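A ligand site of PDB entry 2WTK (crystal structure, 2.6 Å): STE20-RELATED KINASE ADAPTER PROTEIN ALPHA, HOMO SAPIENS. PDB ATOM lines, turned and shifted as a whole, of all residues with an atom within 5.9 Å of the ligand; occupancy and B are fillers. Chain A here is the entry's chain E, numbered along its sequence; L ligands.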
ATOM      1  N   ILE A  17      11.879  26.036  23.694  1.00  0.00           N
ATOM      2  CA  ILE A  17      11.205  27.327  23.636  1.00  0.00           C
ATOM      3  C   ILE A  17      10.006  27.378  24.568  1.00  0.00           C
ATOM      4  O   ILE A  17       9.424  28.449  24.767  1.00  0.00           O
ATOM      5  CB  ILE A  17      10.815  27.756  22.192  1.00  0.00           C
ATOM      6  CG1 ILE A  17       9.931  26.703  21.505  1.00  0.00           C
ATOM      7  CG2 ILE A  17      12.041  28.004  21.359  1.00  0.00           C
ATOM      8  CD1 ILE A  17       9.063  27.268  20.343  1.00  0.00           C
ATOM      9  N   GLY A  18       9.626  26.226  25.139  1.00  0.00           N
ATOM     10  CA  GLY A  18       8.534  26.153  26.108  1.00  0.00           C
ATOM     11  C   GLY A  18       8.261  24.736  26.590  1.00  0.00           C
ATOM     12  O   GLY A  18       8.842  23.779  26.079  1.00  0.00           O
ATOM     13  N   LYS A  19       7.386  24.604  27.587  1.00  0.00           N
ATOM     14  CA  LYS A  19       6.972  23.291  28.084  1.00  0.00           C
ATOM     15  C   LYS A  19       5.457  23.273  28.287  1.00  0.00           C
ATOM     16  O   LYS A  19       4.769  24.233  27.910  1.00  0.00           O
ATOM     17  CB  LYS A  19       7.753  22.887  29.358  1.00  0.00           C
ATOM     18  CG  LYS A  19       7.429  23.680  30.631  1.00  0.00           C
ATOM     19  CD  LYS A  19       8.480  23.491  31.737  1.00  0.00           C
ATOM     20  CE  LYS A  19       8.099  24.266  33.009  1.00  0.00           C
ATOM     21  NZ  LYS A  19       9.080  24.126  34.151  1.00  0.00           N
ATOM     22  N   GLY A  20       4.910  22.191  28.831  1.00  0.00           N
ATOM     23  CA  GLY A  20       3.464  22.130  29.051  1.00  0.00           C
ATOM     24  C   GLY A  20       2.918  20.743  29.262  1.00  0.00           C
ATOM     25  O   GLY A  20       3.676  19.791  29.379  1.00  0.00           O
ATOM     26  N   PHE A  21       1.590  20.644  29.290  1.00  0.00           N
ATOM     27  CA  PHE A  21       0.878  19.386  29.565  1.00  0.00           C
ATOM     28  C   PHE A  21       1.539  18.626  30.707  1.00  0.00           C
ATOM     29  O   PHE A  21       2.231  17.632  30.493  1.00  0.00           O
ATOM     30  CB  PHE A  21       0.748  18.526  28.286  1.00  0.00           C
ATOM     31  CG  PHE A  21      -0.255  17.401  28.403  1.00  0.00           C
ATOM     32  CD1 PHE A  21      -1.582  17.652  28.815  1.00  0.00           C
ATOM     33  CD2 PHE A  21       0.104  16.075  28.090  1.00  0.00           C
ATOM     34  CE1 PHE A  21      -2.525  16.606  28.911  1.00  0.00           C
ATOM     35  CE2 PHE A  21      -0.823  15.028  28.180  1.00  0.00           C
ATOM     36  CZ  PHE A  21      -2.140  15.297  28.600  1.00  0.00           C
ATOM     37  N   GLU A  22       1.366  19.146  31.921  1.00  0.00           N
ATOM     38  CA  GLU A  22       1.889  18.520  33.135  1.00  0.00           C
ATOM     39  C   GLU A  22       3.428  18.300  33.096  1.00  0.00           C
ATOM     40  O   GLU A  22       3.975  17.593  33.946  1.00  0.00           O
ATOM     41  CB  GLU A  22       1.154  17.192  33.429  1.00  0.00           C
ATOM     42  CG  GLU A  22      -0.348  17.145  33.032  1.00  0.00           C
ATOM     43  CD  GLU A  22      -1.316  17.644  34.121  1.00  0.00           C
ATOM     44  OE1 GLU A  22      -1.375  18.871  34.348  1.00  0.00           O
ATOM     45  OE2 GLU A  22      -2.030  16.796  34.723  1.00  0.00           O
ATOM     46  N   MET A  25       5.283  17.477  27.872  1.00  0.00           N
ATOM     47  CA  MET A  25       5.537  18.117  26.578  1.00  0.00           C
ATOM     48  C   MET A  25       6.727  19.081  26.662  1.00  0.00           C
ATOM     49  O   MET A  25       6.752  19.962  27.528  1.00  0.00           O
ATOM     50  CB  MET A  25       4.308  18.921  26.156  1.00  0.00           C
ATOM     51  CG  MET A  25       4.472  19.578  24.803  1.00  0.00           C
ATOM     52  SD  MET A  25       3.080  20.489  24.097  1.00  0.00           S
ATOM     53  CE  MET A  25       3.323  22.178  24.701  1.00  0.00           C
ATOM     54  N   VAL A  27       8.571  21.979  24.231  1.00  0.00           N
ATOM     55  CA  VAL A  27       8.428  22.728  22.964  1.00  0.00           C
ATOM     56  C   VAL A  27       9.825  23.062  22.458  1.00  0.00           C
ATOM     57  O   VAL A  27      10.676  23.638  23.178  1.00  0.00           O
ATOM     58  CB  VAL A  27       7.505  24.005  23.062  1.00  0.00           C
ATOM     59  CG1 VAL A  27       7.238  24.576  21.708  1.00  0.00           C
ATOM     60  CG2 VAL A  27       6.187  23.683  23.680  1.00  0.00           C
ATOM     61  N   THR A  40       8.264  24.867  14.896  1.00  0.00           N
ATOM     62  CA  THR A  40       8.116  24.419  16.255  1.00  0.00           C
ATOM     63  C   THR A  40       7.801  22.919  16.205  1.00  0.00           C
ATOM     64  O   THR A  40       7.006  22.482  15.386  1.00  0.00           O
ATOM     65  CB  THR A  40       6.969  25.196  16.934  1.00  0.00           C
ATOM     66  OG1 THR A  40       7.228  26.599  16.845  1.00  0.00           O
ATOM     67  CG2 THR A  40       6.842  24.842  18.377  1.00  0.00           C
ATOM     68  N   ARG A  42       6.438  20.118  18.907  1.00  0.00           N
ATOM     69  CA  ARG A  42       5.859  19.878  20.223  1.00  0.00           C
ATOM     70  C   ARG A  42       5.929  18.373  20.449  1.00  0.00           C
ATOM     71  O   ARG A  42       5.450  17.608  19.601  1.00  0.00           O
ATOM     72  CB  ARG A  42       4.382  20.316  20.224  1.00  0.00           C
ATOM     73  CG  ARG A  42       4.170  21.742  19.722  1.00  0.00           C
ATOM     74  CD  ARG A  42       2.704  21.998  19.414  1.00  0.00           C
ATOM     75  NE  ARG A  42       1.835  21.905  20.589  1.00  0.00           N
ATOM     76  CZ  ARG A  42       1.722  22.831  21.549  1.00  0.00           C
ATOM     77  NH1 ARG A  42       2.453  23.955  21.531  1.00  0.00           N
ATOM     78  NH2 ARG A  42       0.893  22.599  22.576  1.00  0.00           N
ATOM     79  N   VAL A  73      -3.350  29.529  15.291  1.00  0.00           N
ATOM     80  CA  VAL A  73      -2.142  28.809  14.924  1.00  0.00           C
ATOM     81  C   VAL A  73      -2.496  27.465  14.266  1.00  0.00           C
ATOM     82  O   VAL A  73      -3.145  26.631  14.896  1.00  0.00           O
ATOM     83  CB  VAL A  73      -1.173  28.634  16.131  1.00  0.00           C
ATOM     84  CG1 VAL A  73      -1.883  27.983  17.333  1.00  0.00           C
ATOM     85  CG2 VAL A  73       0.078  27.862  15.720  1.00  0.00           C
ATOM     86  N   THR A  89       4.401  22.803  14.101  1.00  0.00           N
ATOM     87  CA  THR A  89       3.654  24.050  13.900  1.00  0.00           C
ATOM     88  C   THR A  89       4.629  25.151  13.436  1.00  0.00           C
ATOM     89  O   THR A  89       5.856  25.027  13.614  1.00  0.00           O
ATOM     90  CB  THR A  89       2.854  24.520  15.179  1.00  0.00           C
ATOM     91  OG1 THR A  89       3.748  24.872  16.231  1.00  0.00           O
ATOM     92  CG2 THR A  89       1.912  23.437  15.703  1.00  0.00           C
ATOM     93  N   SER A  90       4.095  26.209  12.840  1.00  0.00           N
ATOM     94  CA  SER A  90       4.926  27.359  12.466  1.00  0.00           C
ATOM     95  C   SER A  90       5.576  28.019  13.680  1.00  0.00           C
ATOM     96  O   SER A  90       5.021  27.985  14.782  1.00  0.00           O
ATOM     97  CB  SER A  90       4.134  28.378  11.675  1.00  0.00           C
ATOM     98  OG  SER A  90       4.241  28.054  10.310  1.00  0.00           O
ATOM     99  N   PHE A  91       6.756  28.586  13.473  1.00  0.00           N
ATOM    100  CA  PHE A  91       7.461  29.251  14.535  1.00  0.00           C
ATOM    101  C   PHE A  91       6.965  30.673  14.667  1.00  0.00           C
ATOM    102  O   PHE A  91       7.076  31.453  13.731  1.00  0.00           O
ATOM    103  CB  PHE A  91       8.976  29.227  14.303  1.00  0.00           C
ATOM    104  CG  PHE A  91       9.766  29.989  15.347  1.00  0.00           C
ATOM    105  CD1 PHE A  91       9.685  29.628  16.707  1.00  0.00           C
ATOM    106  CD2 PHE A  91      10.589  31.030  14.989  1.00  0.00           C
ATOM    107  CE1 PHE A  91      10.401  30.314  17.688  1.00  0.00           C
ATOM    108  CE2 PHE A  91      11.321  31.729  15.958  1.00  0.00           C
ATOM    109  CZ  PHE A  91      11.233  31.360  17.319  1.00  0.00           C
ATOM    110  N   MET A  92       6.419  31.002  15.838  1.00  0.00           N
ATOM    111  CA  MET A  92       6.111  32.383  16.204  1.00  0.00           C
ATOM    112  C   MET A  92       7.316  33.017  16.920  1.00  0.00           C
ATOM    113  O   MET A  92       7.566  32.743  18.102  1.00  0.00           O
ATOM    114  CB  MET A  92       4.819  32.434  17.015  1.00  0.00           C
ATOM    115  CG  MET A  92       3.684  31.717  16.309  1.00  0.00           C
ATOM    116  SD  MET A  92       3.543  32.331  14.601  1.00  0.00           S
ATOM    117  CE  MET A  92       2.348  31.181  13.890  1.00  0.00           C
ATOM    118  N   ALA A  93       8.037  33.860  16.187  1.00  0.00           N
ATOM    119  CA  ALA A  93       9.379  34.326  16.587  1.00  0.00           C
ATOM    120  C   ALA A  93       9.406  35.179  17.844  1.00  0.00           C
ATOM    121  O   ALA A  93      10.399  35.169  18.562  1.00  0.00           O
ATOM    122  CB  ALA A  93      10.071  35.060  15.427  1.00  0.00           C
ATOM    123  N   GLY A  95       7.450  34.688  20.302  1.00  0.00           N
ATOM    124  CA  GLY A  95       7.019  33.807  21.359  1.00  0.00           C
ATOM    125  C   GLY A  95       5.594  34.109  21.741  1.00  0.00           C
ATOM    126  O   GLY A  95       4.840  34.682  20.972  1.00  0.00           O
ATOM    127  N   SER A  96       5.195  33.695  22.937  1.00  0.00           N
ATOM    128  CA  SER A  96       3.847  34.032  23.399  1.00  0.00           C
ATOM    129  C   SER A  96       3.933  35.369  24.115  1.00  0.00           C
ATOM    130  O   SER A  96       5.037  35.875  24.386  1.00  0.00           O
ATOM    131  CB  SER A  96       3.228  32.939  24.293  1.00  0.00           C
ATOM    132  OG  SER A  96       3.331  33.272  25.669  1.00  0.00           O
ATOM    133  N   LYS A  98       3.056  35.782  27.102  1.00  0.00           N
ATOM    134  CA  LYS A  98       3.627  35.502  28.415  1.00  0.00           C
ATOM    135  C   LYS A  98       5.154  35.605  28.386  1.00  0.00           C
ATOM    136  O   LYS A  98       5.742  36.171  29.312  1.00  0.00           O
ATOM    137  CB  LYS A  98       3.169  34.157  29.010  1.00  0.00           C
ATOM    138  CG  LYS A  98       3.466  33.993  30.524  1.00  0.00           C
ATOM    139  CD  LYS A  98       2.685  35.029  31.363  1.00  0.00           C
ATOM    140  CE  LYS A  98       2.799  34.807  32.872  1.00  0.00           C
ATOM    141  NZ  LYS A  98       1.847  35.665  33.631  1.00  0.00           N
ATOM    142  N   ASP A  99       5.775  35.107  27.315  1.00  0.00           N
ATOM    143  CA  ASP A  99       7.201  35.339  27.091  1.00  0.00           C
ATOM    144  C   ASP A  99       7.536  36.827  27.186  1.00  0.00           C
ATOM    145  O   ASP A  99       8.330  37.229  28.029  1.00  0.00           O
ATOM    146  CB  ASP A  99       7.674  34.755  25.745  1.00  0.00           C
ATOM    147  CG  ASP A  99       7.442  33.273  25.649  1.00  0.00           C
ATOM    148  OD1 ASP A  99       7.896  32.559  26.571  1.00  0.00           O
ATOM    149  OD2 ASP A  99       6.777  32.817  24.667  1.00  0.00           O
ATOM    150  N   LYS A 139      -5.509  32.612  27.883  1.00  0.00           N
ATOM    151  CA  LYS A 139      -4.483  33.126  28.785  1.00  0.00           C
ATOM    152  C   LYS A 139      -3.288  33.554  27.930  1.00  0.00           C
ATOM    153  O   LYS A 139      -3.136  33.085  26.791  1.00  0.00           O
ATOM    154  CB  LYS A 139      -4.082  32.093  29.852  1.00  0.00           C
ATOM    155  CG  LYS A 139      -3.170  30.982  29.365  1.00  0.00           C
ATOM    156  CD  LYS A 139      -3.164  29.780  30.295  1.00  0.00           C
ATOM    157  CE  LYS A 139      -1.892  29.644  31.131  1.00  0.00           C
ATOM    158  NZ  LYS A 139      -1.632  28.180  31.373  1.00  0.00           N
ATOM    159  N   ALA A 140      -2.466  34.449  28.476  1.00  0.00           N
ATOM    160  CA  ALA A 140      -1.367  35.083  27.736  1.00  0.00           C
ATOM    161  C   ALA A 140      -0.345  34.084  27.187  1.00  0.00           C
ATOM    162  O   ALA A 140       0.215  34.284  26.103  1.00  0.00           O
ATOM    163  CB  ALA A 140      -0.671  36.138  28.593  1.00  0.00           C
ATOM    164  N   SER A 141      -0.117  33.006  27.934  1.00  0.00           N
ATOM    165  CA  SER A 141       0.779  31.951  27.475  1.00  0.00           C
ATOM    166  C   SER A 141       0.217  31.264  26.200  1.00  0.00           C
ATOM    167  O   SER A 141       0.976  30.643  25.433  1.00  0.00           O
ATOM    168  CB  SER A 141       1.074  30.945  28.609  1.00  0.00           C
ATOM    169  OG  SER A 141       0.304  29.752  28.516  1.00  0.00           O
ATOM    170  N   HIS A 142      -1.090  31.396  25.959  1.00  0.00           N
ATOM    171  CA  HIS A 142      -1.671  30.897  24.719  1.00  0.00           C
ATOM    172  C   HIS A 142      -1.878  31.996  23.692  1.00  0.00           C
ATOM    173  O   HIS A 142      -2.835  31.943  22.909  1.00  0.00           O
ATOM    174  CB  HIS A 142      -2.981  30.102  24.946  1.00  0.00           C
ATOM    175  CG  HIS A 142      -2.794  28.812  25.702  1.00  0.00           C
ATOM    176  ND1 HIS A 142      -3.791  28.224  26.448  1.00  0.00           N
ATOM    177  CD2 HIS A 142      -1.704  28.017  25.838  1.00  0.00           C
ATOM    178  CE1 HIS A 142      -3.321  27.124  27.004  1.00  0.00           C
ATOM    179  NE2 HIS A 142      -2.062  26.974  26.644  1.00  0.00           N
ATOM    180  N   LEU A 144       0.282  33.819  20.627  1.00  0.00           N
ATOM    181  CA  LEU A 144       1.543  33.856  19.929  1.00  0.00           C
ATOM    182  C   LEU A 144       1.617  35.027  18.968  1.00  0.00           C
ATOM    183  O   LEU A 144       0.696  35.244  18.187  1.00  0.00           O
ATOM    184  CB  LEU A 144       1.797  32.537  19.208  1.00  0.00           C
ATOM    185  CG  LEU A 144       1.610  31.265  20.044  1.00  0.00           C
ATOM    186  CD1 LEU A 144       1.945  30.040  19.238  1.00  0.00           C
ATOM    187  CD2 LEU A 144       2.460  31.297  21.314  1.00  0.00           C
ATOM    188  N   SER A 154      -3.599  30.098  20.690  1.00  0.00           N
ATOM    189  CA  SER A 154      -3.259  28.667  20.755  1.00  0.00           C
ATOM    190  C   SER A 154      -4.063  27.953  21.848  1.00  0.00           C
ATOM    191  O   SER A 154      -5.202  28.307  22.106  1.00  0.00           O
ATOM    192  CB  SER A 154      -1.741  28.441  20.879  1.00  0.00           C
ATOM    193  OG  SER A 154      -1.169  29.042  22.033  1.00  0.00           O
ATOM    194  N   GLY A 155      -3.489  26.929  22.467  1.00  0.00           N
ATOM    195  CA  GLY A 155      -4.180  26.211  23.533  1.00  0.00           C
ATOM    196  C   GLY A 155      -5.419  25.436  23.104  1.00  0.00           C
ATOM    197  O   GLY A 155      -6.360  25.337  23.865  1.00  0.00           O
ATOM    198  N   ARG A 157      -5.894  22.359  22.973  1.00  0.00           N
ATOM    199  CA  ARG A 157      -6.027  21.153  23.759  1.00  0.00           C
ATOM    200  C   ARG A 157      -7.262  21.181  24.676  1.00  0.00           C
ATOM    201  O   ARG A 157      -7.904  20.148  24.913  1.00  0.00           O
ATOM    202  CB  ARG A 157      -4.763  20.943  24.563  1.00  0.00           C
ATOM    203  CG  ARG A 157      -4.598  19.559  25.101  1.00  0.00           C
ATOM    204  CD  ARG A 157      -3.505  19.513  26.156  1.00  0.00           C
ATOM    205  NE  ARG A 157      -2.204  19.626  25.510  1.00  0.00           N
ATOM    206  CZ  ARG A 157      -1.194  20.348  25.993  1.00  0.00           C
ATOM    207  NH1 ARG A 157      -1.365  21.039  27.121  1.00  0.00           N
ATOM    208  NH2 ARG A 157      -0.034  20.381  25.341  1.00  0.00           N
ATOM    209  N   LYS A 181      -3.163  24.528  36.080  1.00  0.00           N
ATOM    210  CA  LYS A 181      -2.492  25.801  35.753  1.00  0.00           C
ATOM    211  C   LYS A 181      -3.475  26.882  35.322  1.00  0.00           C
ATOM    212  O   LYS A 181      -3.378  28.037  35.729  1.00  0.00           O
ATOM    213  CB  LYS A 181      -1.400  25.606  34.704  1.00  0.00           C
ATOM    214  CG  LYS A 181      -0.334  24.598  35.113  1.00  0.00           C
ATOM    215  CD  LYS A 181       1.038  24.916  34.515  1.00  0.00           C
ATOM    216  CE  LYS A 181       2.150  24.137  35.268  1.00  0.00           C
ATOM    217  NZ  LYS A 181       3.495  24.804  35.213  1.00  0.00           N
ATOM    218  N   VAL A 182      -4.448  26.488  34.505  1.00  0.00           N
ATOM    219  CA  VAL A 182      -5.442  27.409  33.939  1.00  0.00           C
ATOM    220  C   VAL A 182      -6.410  28.007  34.969  1.00  0.00           C
ATOM    221  O   VAL A 182      -6.881  29.131  34.784  1.00  0.00           O
ATOM    222  CB  VAL A 182      -6.187  26.739  32.754  1.00  0.00           C
ATOM    223  CG1 VAL A 182      -7.417  27.529  32.315  1.00  0.00           C
ATOM    224  CG2 VAL A 182      -5.226  26.549  31.581  1.00  0.00           C
ATOM    225  N   PHE A 357      13.506  34.352  23.041  1.00  0.00           N
ATOM    226  CA  PHE A 357      12.498  35.398  23.241  1.00  0.00           C
ATOM    227  C   PHE A 357      13.029  36.528  24.139  1.00  0.00           C
ATOM    228  O   PHE A 357      13.920  36.316  24.976  1.00  0.00           O
ATOM    229  CB  PHE A 357      11.170  34.831  23.801  1.00  0.00           C
ATOM    230  CG  PHE A 357      10.676  33.584  23.083  1.00  0.00           C
ATOM    231  CD1 PHE A 357      10.571  33.537  21.700  1.00  0.00           C
ATOM    232  CD2 PHE A 357      10.300  32.456  23.814  1.00  0.00           C
ATOM    233  CE1 PHE A 357      10.115  32.383  21.060  1.00  0.00           C
ATOM    234  CE2 PHE A 357       9.840  31.304  23.160  1.00  0.00           C
ATOM    235  CZ  PHE A 357       9.753  31.257  21.795  1.00  0.00           C
HETATM  236  P1  LIG L   1       0.812  25.270  29.910  1.00  0.00           P
HETATM  237  O1  LIG L   1       1.743  25.097  31.092  1.00  0.00           O
HETATM  238  O2  LIG L   1      -0.324  24.272  29.924  1.00  0.00           O
HETATM  239  O3  LIG L   1       0.426  26.715  29.600  1.00  0.00           O
HETATM  240  P2  LIG L   1       0.890  24.160  27.151  1.00  0.00           P
HETATM  241  O4  LIG L   1       0.819  22.660  27.295  1.00  0.00           O
HETATM  242  O5  LIG L   1      -0.421  24.883  27.079  1.00  0.00           O
HETATM  243  N1  LIG L   1       1.745  24.808  28.516  1.00  0.00           N
HETATM  244  P3  LIG L   1       1.730  25.707  24.898  1.00  0.00           P
HETATM  245  O6  LIG L   1       1.099  25.309  23.593  1.00  0.00           O
HETATM  246  O7  LIG L   1       1.242  26.888  25.692  1.00  0.00           O
HETATM  247  O8  LIG L   1       1.784  24.388  25.833  1.00  0.00           O
HETATM  248  O9  LIG L   1       3.279  25.984  24.576  1.00  0.00           O
HETATM  249  C1  LIG L   1       4.090  26.384  25.684  1.00  0.00           C
HETATM  250  C2  LIG L   1       4.899  27.606  25.320  1.00  0.00           C
HETATM  251  O10 LIG L   1       5.758  27.312  24.230  1.00  0.00           O
HETATM  252  C3  LIG L   1       4.106  28.826  24.868  1.00  0.00           C
HETATM  253  O11 LIG L   1       3.578  29.612  25.941  1.00  0.00           O
HETATM  254  C4  LIG L   1       5.181  29.572  24.122  1.00  0.00           C
HETATM  255  O12 LIG L   1       5.982  30.227  25.109  1.00  0.00           O
HETATM  256  C5  LIG L   1       5.972  28.477  23.443  1.00  0.00           C
HETATM  257  N2  LIG L   1       5.458  28.172  22.086  1.00  0.00           N
HETATM  258  C6  LIG L   1       4.532  27.240  21.753  1.00  0.00           C
HETATM  259  N3  LIG L   1       4.279  27.203  20.418  1.00  0.00           N
HETATM  260  C7  LIG L   1       5.065  28.138  19.852  1.00  0.00           C
HETATM  261  C8  LIG L   1       5.330  28.659  18.483  1.00  0.00           C
HETATM  262  N4  LIG L   1       4.679  28.157  17.422  1.00  0.00           N
HETATM  263  N5  LIG L   1       6.246  29.643  18.333  1.00  0.00           N
HETATM  264  C9  LIG L   1       6.915  30.181  19.387  1.00  0.00           C
HETATM  265  N6  LIG L   1       6.727  29.769  20.652  1.00  0.00           N
HETATM  266  C10 LIG L   1       5.846  28.769  20.953  1.00  0.00           C
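The backbone carbonyl oxygen (O) of Ser 90 sits at hydrogen-bond distance from a nitrogen (N4) of the ligand, 2.7 Å away. NE2 of His 142 sits at hydrogen-bond distance from O5 of the ligand, 2.7 Å away. The guanidinium group (NH1) of Arg 157 lies within salt-bridge range of an oxygen (O4) of the ligand, at 2.7 Å. OD2 of Asp 99 lies within hydrogen-bond range of O12 of the ligand (2.7 Å). The guanidinium group (NH1) of Arg 42 lies within salt-bridge range of an oxygen (O6) of the ligand (2.8 Å). O11 of the ligand sits at hydrogen-bond distance from O of Ser 141, at 2.8 Å. An oxygen (O3) of the ligand is in hydrogen-bond range of the side-chain hydroxyl of Ser 141, 3.2 Å away. A nitrogen (N5) of the ligand is in hydrogen-bond range of the backbone NH (N) of Met 92 (2.8 Å). O4 of the ligand is in hydrogen-bond range of N of Phe 21. N4 of the ligand lies within hydrogen-bond range of OG1 of Thr 40, at 3.0 Å. The side-chain amino group of Lys 139 is in salt-bridge range of an oxygen (O3) of the ligand (3.1 Å). O of Lys 19 sits at hydrogen-bond distance from N1 of the ligand, 3.1 Å away.
The backbone carbonyl oxygen of Ser 90 sits at hydrogen-bond distance from the side-chain hydroxyl of Thr 40 (3.3 Å). The backbone carbonyl oxygen (O) of His 142 sits at hydrogen-bond distance from the backbone NH (N) of Ser 154. The guanidinium group of Arg 157 lies within hydrogen-bond range of the side-chain sulfur of Met 25 (3.4 Å). The side-chain carboxylate (OD2) of Asp 99 lies within hydrogen-bond range of the backbone NH (N) of Ser 96. The guanidinium group (NH2) of Arg 42 lies close to the side-chain sulfur (SD) of Met 25. N of Ile 17 lies within hydrogen-bond range of O of Val 27. The side-chain hydroxyl (OG) of Ser 96 sits at hydrogen-bond distance from the backbone NH (N) of Lys 98, 2.9 Å away. The side-chain hydroxyl of Ser 96 sits at hydrogen-bond distance from the backbone carbonyl oxygen of Ala 140 (3.3 Å).
Residues that only touch the ligand: Met 25 (2.9 Å), Gly 20 (3.2 Å), Ile 17 (3.4 Å), Lys 181 (3.5 Å), Gly 18 (3.5 Å), Phe 357 (3.6 Å), Thr 89 (3.6 Å), Ser 96 (3.7 Å), Val 27 (3.7 Å), Leu 144 (3.7 Å) and Phe 91 (3.8 Å). Hydrophobic or aromatic side chains within 4 Å of the ligand: Ile 17, Met 25, Val 27, Phe 91, Met 92, His 142, Leu 144 and Phe 357. Within 4 Å of the ligand: Ile 17, Gly 18, Lys 19, Gly 20, Phe 21, Met 25, Val 27, Thr 40, Arg 42, Thr 89, Ser 90, Phe 91, Met 92, Ser 96, Asp 99, Lys 139, Ser 141, His 142, Leu 144, Arg 157, Lys 181 and Phe 357. Along chain A the residues within 4 Å of the ligand span positions 17 to 357.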
